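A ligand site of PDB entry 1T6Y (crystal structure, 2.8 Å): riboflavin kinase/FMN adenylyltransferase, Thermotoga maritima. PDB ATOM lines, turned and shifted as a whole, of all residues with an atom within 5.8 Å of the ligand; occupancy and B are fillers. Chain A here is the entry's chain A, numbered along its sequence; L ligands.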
ATOM      1  N   PHE A 178       3.567  -8.458   8.297  1.00  0.00           N
ATOM      2  CA  PHE A 178       4.752  -7.993   8.991  1.00  0.00           C
ATOM      3  C   PHE A 178       5.967  -8.075   8.066  1.00  0.00           C
ATOM      4  O   PHE A 178       6.831  -7.196   8.096  1.00  0.00           O
ATOM      5  CB  PHE A 178       4.952  -8.822  10.262  1.00  0.00           C
ATOM      6  CG  PHE A 178       6.011  -8.284  11.199  1.00  0.00           C
ATOM      7  CD1 PHE A 178       6.086  -8.741  12.512  1.00  0.00           C
ATOM      8  CD2 PHE A 178       6.949  -7.341  10.764  1.00  0.00           C
ATOM      9  CE1 PHE A 178       7.084  -8.285  13.380  1.00  0.00           C
ATOM     10  CE2 PHE A 178       7.944  -6.874  11.610  1.00  0.00           C
ATOM     11  CZ  PHE A 178       8.015  -7.344  12.922  1.00  0.00           C
ATOM     12  N   PRO A 179       6.071  -9.131   7.232  1.00  0.00           N
ATOM     13  CA  PRO A 179       5.163 -10.269   7.070  1.00  0.00           C
ATOM     14  C   PRO A 179       5.809 -11.439   7.774  1.00  0.00           C
ATOM     15  O   PRO A 179       6.973 -11.371   8.193  1.00  0.00           O
ATOM     16  CB  PRO A 179       5.119 -10.474   5.545  1.00  0.00           C
ATOM     17  CG  PRO A 179       5.962  -9.330   4.962  1.00  0.00           C
ATOM     18  CD  PRO A 179       6.944  -9.037   6.057  1.00  0.00           C
ATOM     19  N   THR A 180       5.045 -12.512   7.880  1.00  0.00           N
ATOM     20  CA  THR A 180       5.510 -13.713   8.532  1.00  0.00           C
ATOM     21  C   THR A 180       5.134 -14.891   7.641  1.00  0.00           C
ATOM     22  O   THR A 180       4.088 -14.900   7.017  1.00  0.00           O
ATOM     23  CB  THR A 180       4.854 -13.875   9.906  1.00  0.00           C
ATOM     24  OG1 THR A 180       3.449 -14.135   9.751  1.00  0.00           O
ATOM     25  CG2 THR A 180       5.050 -12.606  10.716  1.00  0.00           C
ATOM     26  N   VAL A 197       8.123 -16.819  21.221  1.00  0.00           N
ATOM     27  CA  VAL A 197       8.956 -16.244  20.179  1.00  0.00           C
ATOM     28  C   VAL A 197      10.331 -16.869  20.248  1.00  0.00           C
ATOM     29  O   VAL A 197      10.921 -17.002  21.326  1.00  0.00           O
ATOM     30  CB  VAL A 197       9.101 -14.732  20.344  1.00  0.00           C
ATOM     31  CG1 VAL A 197       9.830 -14.146  19.143  1.00  0.00           C
ATOM     32  CG2 VAL A 197       7.725 -14.107  20.497  1.00  0.00           C
ATOM     33  N   VAL A 213      12.869 -14.553  13.219  1.00  0.00           N
ATOM     34  CA  VAL A 213      12.188 -14.701  14.496  1.00  0.00           C
ATOM     35  C   VAL A 213      10.897 -15.442  14.202  1.00  0.00           C
ATOM     36  O   VAL A 213      10.188 -15.135  13.224  1.00  0.00           O
ATOM     37  CB  VAL A 213      11.869 -13.354  15.141  1.00  0.00           C
ATOM     38  CG1 VAL A 213      11.993 -13.478  16.638  1.00  0.00           C
ATOM     39  CG2 VAL A 213      12.801 -12.285  14.620  1.00  0.00           C
ATOM     40  N   MET A 214      10.597 -16.430  15.037  1.00  0.00           N
ATOM     41  CA  MET A 214       9.435 -17.264  14.841  1.00  0.00           C
ATOM     42  C   MET A 214       8.542 -17.337  16.066  1.00  0.00           C
ATOM     43  O   MET A 214       8.988 -17.701  17.154  1.00  0.00           O
ATOM     44  CB  MET A 214       9.904 -18.671  14.440  1.00  0.00           C
ATOM     45  CG  MET A 214       8.809 -19.716  14.362  1.00  0.00           C
ATOM     46  SD  MET A 214       9.360 -21.437  14.407  1.00  0.00           S
ATOM     47  CE  MET A 214      10.386 -21.479  15.970  1.00  0.00           C
ATOM     48  N   ASN A 215       7.267 -17.000  15.904  1.00  0.00           N
ATOM     49  CA  ASN A 215       6.348 -17.086  17.023  1.00  0.00           C
ATOM     50  C   ASN A 215       5.453 -18.314  16.882  1.00  0.00           C
ATOM     51  O   ASN A 215       5.148 -18.755  15.768  1.00  0.00           O
ATOM     52  CB  ASN A 215       5.498 -15.822  17.128  1.00  0.00           C
ATOM     53  CG  ASN A 215       4.380 -15.986  18.136  1.00  0.00           C
ATOM     54  OD1 ASN A 215       3.296 -16.481  17.808  1.00  0.00           O
ATOM     55  ND2 ASN A 215       4.647 -15.602  19.378  1.00  0.00           N
ATOM     56  N   PHE A 218      -1.646 -20.574  19.653  1.00  0.00           N
ATOM     57  CA  PHE A 218      -2.801 -21.478  19.563  1.00  0.00           C
ATOM     58  C   PHE A 218      -3.813 -21.307  18.428  1.00  0.00           C
ATOM     59  O   PHE A 218      -3.797 -20.314  17.677  1.00  0.00           O
ATOM     60  CB  PHE A 218      -3.574 -21.506  20.891  1.00  0.00           C
ATOM     61  CG  PHE A 218      -3.045 -22.511  21.856  1.00  0.00           C
ATOM     62  CD1 PHE A 218      -1.840 -22.302  22.512  1.00  0.00           C
ATOM     63  CD2 PHE A 218      -3.726 -23.695  22.090  1.00  0.00           C
ATOM     64  CE1 PHE A 218      -1.314 -23.256  23.398  1.00  0.00           C
ATOM     65  CE2 PHE A 218      -3.219 -24.666  22.974  1.00  0.00           C
ATOM     66  CZ  PHE A 218      -1.998 -24.432  23.626  1.00  0.00           C
ATOM     67  N   LYS A 229       0.278 -22.624  15.693  1.00  0.00           N
ATOM     68  CA  LYS A 229       0.732 -22.037  14.431  1.00  0.00           C
ATOM     69  C   LYS A 229       2.187 -21.639  14.499  1.00  0.00           C
ATOM     70  O   LYS A 229       2.689 -21.270  15.568  1.00  0.00           O
ATOM     71  CB  LYS A 229      -0.067 -20.798  14.063  1.00  0.00           C
ATOM     72  CG  LYS A 229      -1.340 -21.058  13.291  1.00  0.00           C
ATOM     73  CD  LYS A 229      -1.649 -19.900  12.330  1.00  0.00           C
ATOM     74  CE  LYS A 229      -1.635 -18.523  13.005  1.00  0.00           C
ATOM     75  NZ  LYS A 229      -1.943 -17.440  12.033  1.00  0.00           N
ATOM     76  N   GLU A 231       4.878 -19.134  12.635  1.00  0.00           N
ATOM     77  CA  GLU A 231       5.095 -18.001  11.759  1.00  0.00           C
ATOM     78  C   GLU A 231       6.491 -17.437  12.065  1.00  0.00           C
ATOM     79  O   GLU A 231       6.868 -17.259  13.237  1.00  0.00           O
ATOM     80  CB  GLU A 231       4.018 -16.922  12.001  1.00  0.00           C
ATOM     81  CG  GLU A 231       2.814 -16.965  11.020  1.00  0.00           C
ATOM     82  CD  GLU A 231       1.509 -16.371  11.599  1.00  0.00           C
ATOM     83  OE1 GLU A 231       0.751 -15.712  10.839  1.00  0.00           O
ATOM     84  OE2 GLU A 231       1.240 -16.581  12.802  1.00  0.00           O
ATOM     85  N   VAL A 232       7.246 -17.169  10.990  1.00  0.00           N
ATOM     86  CA  VAL A 232       8.599 -16.641  11.111  1.00  0.00           C
ATOM     87  C   VAL A 232       8.672 -15.315  10.362  1.00  0.00           C
ATOM     88  O   VAL A 232       8.050 -15.136   9.298  1.00  0.00           O
ATOM     89  CB  VAL A 232       9.663 -17.651  10.471  1.00  0.00           C
ATOM     90  CG1 VAL A 232      10.220 -17.105   9.152  1.00  0.00           C
ATOM     91  CG2 VAL A 232      10.813 -17.923  11.417  1.00  0.00           C
ATOM     92  N   TYR A 233       9.393 -14.350  10.913  1.00  0.00           N
ATOM     93  CA  TYR A 233       9.594 -13.112  10.182  1.00  0.00           C
ATOM     94  C   TYR A 233      11.065 -13.282   9.826  1.00  0.00           C
ATOM     95  O   TYR A 233      11.940 -13.255  10.715  1.00  0.00           O
ATOM     96  CB  TYR A 233       9.401 -11.851  11.032  1.00  0.00           C
ATOM     97  CG  TYR A 233      10.104 -10.661  10.396  1.00  0.00           C
ATOM     98  CD1 TYR A 233       9.607 -10.094   9.211  1.00  0.00           C
ATOM     99  CD2 TYR A 233      11.305 -10.170  10.913  1.00  0.00           C
ATOM    100  CE1 TYR A 233      10.300  -9.086   8.560  1.00  0.00           C
ATOM    101  CE2 TYR A 233      12.004  -9.157  10.268  1.00  0.00           C
ATOM    102  CZ  TYR A 233      11.506  -8.620   9.090  1.00  0.00           C
ATOM    103  OH  TYR A 233      12.207  -7.648   8.409  1.00  0.00           O
ATOM    104  N   ARG A 255      11.191 -15.041  24.289  1.00  0.00           N
ATOM    105  CA  ARG A 255      10.188 -14.639  25.279  1.00  0.00           C
ATOM    106  C   ARG A 255       8.870 -15.395  25.146  1.00  0.00           C
ATOM    107  O   ARG A 255       8.558 -15.969  24.088  1.00  0.00           O
ATOM    108  CB  ARG A 255       9.923 -13.132  25.140  1.00  0.00           C
ATOM    109  CG  ARG A 255       9.043 -12.800  23.949  1.00  0.00           C
ATOM    110  CD  ARG A 255       9.065 -11.317  23.641  1.00  0.00           C
ATOM    111  NE  ARG A 255       8.186 -11.023  22.508  1.00  0.00           N
ATOM    112  CZ  ARG A 255       6.917 -11.408  22.453  1.00  0.00           C
ATOM    113  NH1 ARG A 255       6.401 -12.106  23.479  1.00  0.00           N
ATOM    114  NH2 ARG A 255       6.160 -11.111  21.388  1.00  0.00           N
ATOM    115  N   ASP A 256       8.071 -15.363  26.221  1.00  0.00           N
ATOM    116  CA  ASP A 256       6.779 -16.041  26.274  1.00  0.00           C
ATOM    117  C   ASP A 256       5.679 -15.435  25.400  1.00  0.00           C
ATOM    118  O   ASP A 256       5.732 -14.255  25.045  1.00  0.00           O
ATOM    119  CB  ASP A 256       6.302 -16.128  27.718  1.00  0.00           C
ATOM    120  CG  ASP A 256       7.319 -16.786  28.617  1.00  0.00           C
ATOM    121  OD1 ASP A 256       8.463 -16.258  28.691  1.00  0.00           O
ATOM    122  OD2 ASP A 256       6.997 -17.833  29.234  1.00  0.00           O
ATOM    123  N   GLU A 257       4.698 -16.272  25.076  1.00  0.00           N
ATOM    124  CA  GLU A 257       3.557 -15.878  24.252  1.00  0.00           C
ATOM    125  C   GLU A 257       2.680 -14.864  25.022  1.00  0.00           C
ATOM    126  O   GLU A 257       2.080 -15.213  26.050  1.00  0.00           O
ATOM    127  CB  GLU A 257       2.748 -17.135  23.906  1.00  0.00           C
ATOM    128  CG  GLU A 257       1.653 -16.951  22.874  1.00  0.00           C
ATOM    129  CD  GLU A 257       2.178 -16.390  21.576  1.00  0.00           C
ATOM    130  OE1 GLU A 257       1.360 -16.211  20.641  1.00  0.00           O
ATOM    131  OE2 GLU A 257       3.404 -16.135  21.484  1.00  0.00           O
ATOM    132  N   LYS A 258       2.605 -13.623  24.528  1.00  0.00           N
ATOM    133  CA  LYS A 258       1.846 -12.551  25.203  1.00  0.00           C
ATOM    134  C   LYS A 258       0.527 -12.076  24.590  1.00  0.00           C
ATOM    135  O   LYS A 258       0.255 -12.302  23.413  1.00  0.00           O
ATOM    136  CB  LYS A 258       2.774 -11.340  25.387  1.00  0.00           C
ATOM    137  CG  LYS A 258       2.134 -10.182  26.136  1.00  0.00           C
ATOM    138  CD  LYS A 258       2.995  -8.928  26.118  1.00  0.00           C
ATOM    139  CE  LYS A 258       2.310  -7.795  26.882  1.00  0.00           C
ATOM    140  NZ  LYS A 258       3.096  -6.527  26.833  1.00  0.00           N
ATOM    141  N   LYS A 259      -0.281 -11.407  25.416  1.00  0.00           N
ATOM    142  CA  LYS A 259      -1.591 -10.845  25.061  1.00  0.00           C
ATOM    143  C   LYS A 259      -2.012 -10.983  23.604  1.00  0.00           C
ATOM    144  O   LYS A 259      -2.671 -10.087  23.064  1.00  0.00           O
ATOM    145  CB  LYS A 259      -1.659  -9.354  25.434  1.00  0.00           C
ATOM    146  CG  LYS A 259      -1.600  -9.081  26.928  1.00  0.00           C
ATOM    147  CD  LYS A 259      -2.116  -7.689  27.276  1.00  0.00           C
ATOM    148  CE  LYS A 259      -2.216  -7.518  28.794  1.00  0.00           C
ATOM    149  NZ  LYS A 259      -3.052  -6.355  29.211  1.00  0.00           N
ATOM    150  N   LEU A 266       1.294  -4.761  20.132  1.00  0.00           N
ATOM    151  CA  LEU A 266       2.123  -5.893  19.779  1.00  0.00           C
ATOM    152  C   LEU A 266       3.168  -5.527  18.728  1.00  0.00           C
ATOM    153  O   LEU A 266       4.308  -5.973  18.801  1.00  0.00           O
ATOM    154  CB  LEU A 266       1.256  -7.015  19.250  1.00  0.00           C
ATOM    155  CG  LEU A 266       1.952  -8.372  19.252  1.00  0.00           C
ATOM    156  CD1 LEU A 266       2.170  -8.856  20.697  1.00  0.00           C
ATOM    157  CD2 LEU A 266       1.088  -9.340  18.467  1.00  0.00           C
ATOM    158  N   ILE A 270       7.136  -6.919  19.146  1.00  0.00           N
ATOM    159  CA  ILE A 270       7.952  -7.690  18.228  1.00  0.00           C
ATOM    160  C   ILE A 270       9.314  -7.034  18.058  1.00  0.00           C
ATOM    161  O   ILE A 270      10.326  -7.716  17.925  1.00  0.00           O
ATOM    162  CB  ILE A 270       7.248  -7.830  16.844  1.00  0.00           C
ATOM    163  CG1 ILE A 270       6.885  -6.463  16.272  1.00  0.00           C
ATOM    164  CG2 ILE A 270       5.962  -8.634  16.983  1.00  0.00           C
ATOM    165  CD1 ILE A 270       8.038  -5.705  15.651  1.00  0.00           C
ATOM    166  N   ASP A 273      11.979  -8.089  20.184  1.00  0.00           N
ATOM    167  CA  ASP A 273      12.590  -9.281  19.583  1.00  0.00           C
ATOM    168  C   ASP A 273      13.528  -8.984  18.420  1.00  0.00           C
ATOM    169  O   ASP A 273      14.693  -9.379  18.448  1.00  0.00           O
ATOM    170  CB  ASP A 273      11.492 -10.240  19.115  1.00  0.00           C
ATOM    171  CG  ASP A 273      10.495 -10.560  20.213  1.00  0.00           C
ATOM    172  OD1 ASP A 273      10.938 -11.012  21.288  1.00  0.00           O
ATOM    173  OD2 ASP A 273       9.277 -10.354  19.994  1.00  0.00           O
ATOM    174  N   VAL A 274      13.021  -8.310  17.403  1.00  0.00           N
ATOM    175  CA  VAL A 274      13.823  -7.991  16.230  1.00  0.00           C
ATOM    176  C   VAL A 274      15.091  -7.246  16.654  1.00  0.00           C
ATOM    177  O   VAL A 274      16.214  -7.670  16.352  1.00  0.00           O
ATOM    178  CB  VAL A 274      13.022  -7.134  15.227  1.00  0.00           C
ATOM    179  CG1 VAL A 274      13.864  -6.863  13.986  1.00  0.00           C
ATOM    180  CG2 VAL A 274      11.716  -7.839  14.873  1.00  0.00           C
HETATM  181  N1  LIG L   1       1.362 -12.668  18.687  1.00  0.00           N
HETATM  182  C1  LIG L   1       0.920 -12.779  19.957  1.00  0.00           C
HETATM  183  O1  LIG L   1      -0.238 -12.919  20.356  1.00  0.00           O
HETATM  184  N2  LIG L   1       1.917 -12.754  21.058  1.00  0.00           N
HETATM  185  C2  LIG L   1       3.320 -12.609  20.809  1.00  0.00           C
HETATM  186  O2  LIG L   1       4.031 -12.600  21.823  1.00  0.00           O
HETATM  187  C3  LIG L   1       3.693 -12.512  19.475  1.00  0.00           C
HETATM  188  N3  LIG L   1       4.937 -12.405  19.220  1.00  0.00           N
HETATM  189  C4  LIG L   1       5.382 -12.301  17.891  1.00  0.00           C
HETATM  190  C5  LIG L   1       6.757 -12.195  17.556  1.00  0.00           C
HETATM  191  C6  LIG L   1       7.166 -12.094  16.168  1.00  0.00           C
HETATM  192  C7  LIG L   1       8.687 -11.999  16.107  1.00  0.00           C
HETATM  193  C8  LIG L   1       6.158 -12.105  15.099  1.00  0.00           C
HETATM  194  C9  LIG L   1       6.604 -12.005  13.693  1.00  0.00           C
HETATM  195  C10 LIG L   1       4.820 -12.212  15.415  1.00  0.00           C
HETATM  196  C11 LIG L   1       4.354 -12.320  16.815  1.00  0.00           C
HETATM  197  N4  LIG L   1       3.014 -12.420  17.033  1.00  0.00           N
HETATM  198  C12 LIG L   1       2.644 -12.530  18.342  1.00  0.00           C
HETATM  199  C13 LIG L   1       1.971 -12.402  15.992  1.00  0.00           C
HETATM  200  C14 LIG L   1       0.937 -13.460  15.817  1.00  0.00           C
HETATM  201  O3  LIG L   1       1.590 -14.684  15.560  1.00  0.00           O
HETATM  202  C15 LIG L   1       0.156 -12.923  14.648  1.00  0.00           C
HETATM  203  O4  LIG L   1      -1.079 -12.316  15.133  1.00  0.00           O
HETATM  204  C16 LIG L   1      -0.328 -13.868  13.521  1.00  0.00           C
HETATM  205  O5  LIG L   1      -1.029 -13.133  12.526  1.00  0.00           O
HETATM  206  C17 LIG L   1      -1.194 -15.107  13.927  1.00  0.00           C
HETATM  207  O6  LIG L   1      -1.942 -14.781  15.132  1.00  0.00           O
HETATM  208  P1  LIG L   1      -3.510 -14.862  15.039  1.00  0.00           P
HETATM  209  O7  LIG L   1      -3.992 -14.465  16.468  1.00  0.00           O
HETATM  210  O8  LIG L   1      -3.969 -13.843  14.026  1.00  0.00           O
HETATM  211  O9  LIG L   1      -3.934 -16.318  14.698  1.00  0.00           O
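Phe 178 touches the ligand. Thr 180 touches the ligand (CG2 to C9, 3.4 Å). Val 197 touches the ligand (CG2 to N3, 3.5 Å). Val 213 touches the ligand. CB of Tyr 233 touches C9 of the ligand (3.9 Å). Glu 257 touches the ligand. Leu 266 touches the ligand. Ile 270 touches the ligand (CG2 to C5, 3.7 Å). Asp 273 touches the ligand (OD2 to C5, 3.96 Å). Hydrophobic or aromatic side chains that line the ligand: Phe 178, Val 197, Val 213, Tyr 233, Leu 266 and Ile 270.
The backbone carbonyl oxygen of Arg 255 is in hydrogen-bond range of the backbone NH of Val 197, at 3.0 Å. OD2 of Asp 273 is in salt-bridge range of NE of Arg 255, 2.8 Å away. The side-chain amino group (NZ) of Lys 229 is in salt-bridge range of the side-chain carboxylate (OE2) of Glu 231 (3.4 Å). O of Glu 231 sits at hydrogen-bond distance from N of Asn 215. The side-chain hydroxyl (OG1) of Thr 180 sits close to the side-chain carboxylate (OE1) of Glu 231, at 3.3 Å. OE2 of Glu 257 is in hydrogen-bond range of ND2 of Asn 215 (2.5 Å). The backbone carbonyl oxygen (O) of Val 213 lies within hydrogen-bond range of the backbone NH (N) of Tyr 233, at 2.6 Å.
NH2 of Arg 255 is in hydrogen-bond range of O2 of the ligand, 2.6 Å away. O2 of the ligand sits at hydrogen-bond distance from N of Lys 258 (3.2 Å). A nitrogen (N2) of the ligand lies within hydrogen-bond range of the backbone carbonyl oxygen (O) of Lys 258, 2.9 Å away. The side-chain carboxylate of Glu 231 sits close to an oxygen (O3) of the ligand, at 3.4 Å. The side-chain amino group (NZ) of Lys 229 lies within salt-bridge range of an oxygen (O9) of the ligand, 3.5 Å away. The side-chain amide nitrogen (ND2) of Asn 215 lies within hydrogen-bond range of a nitrogen (N3) of the ligand, 3.2 Å away.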
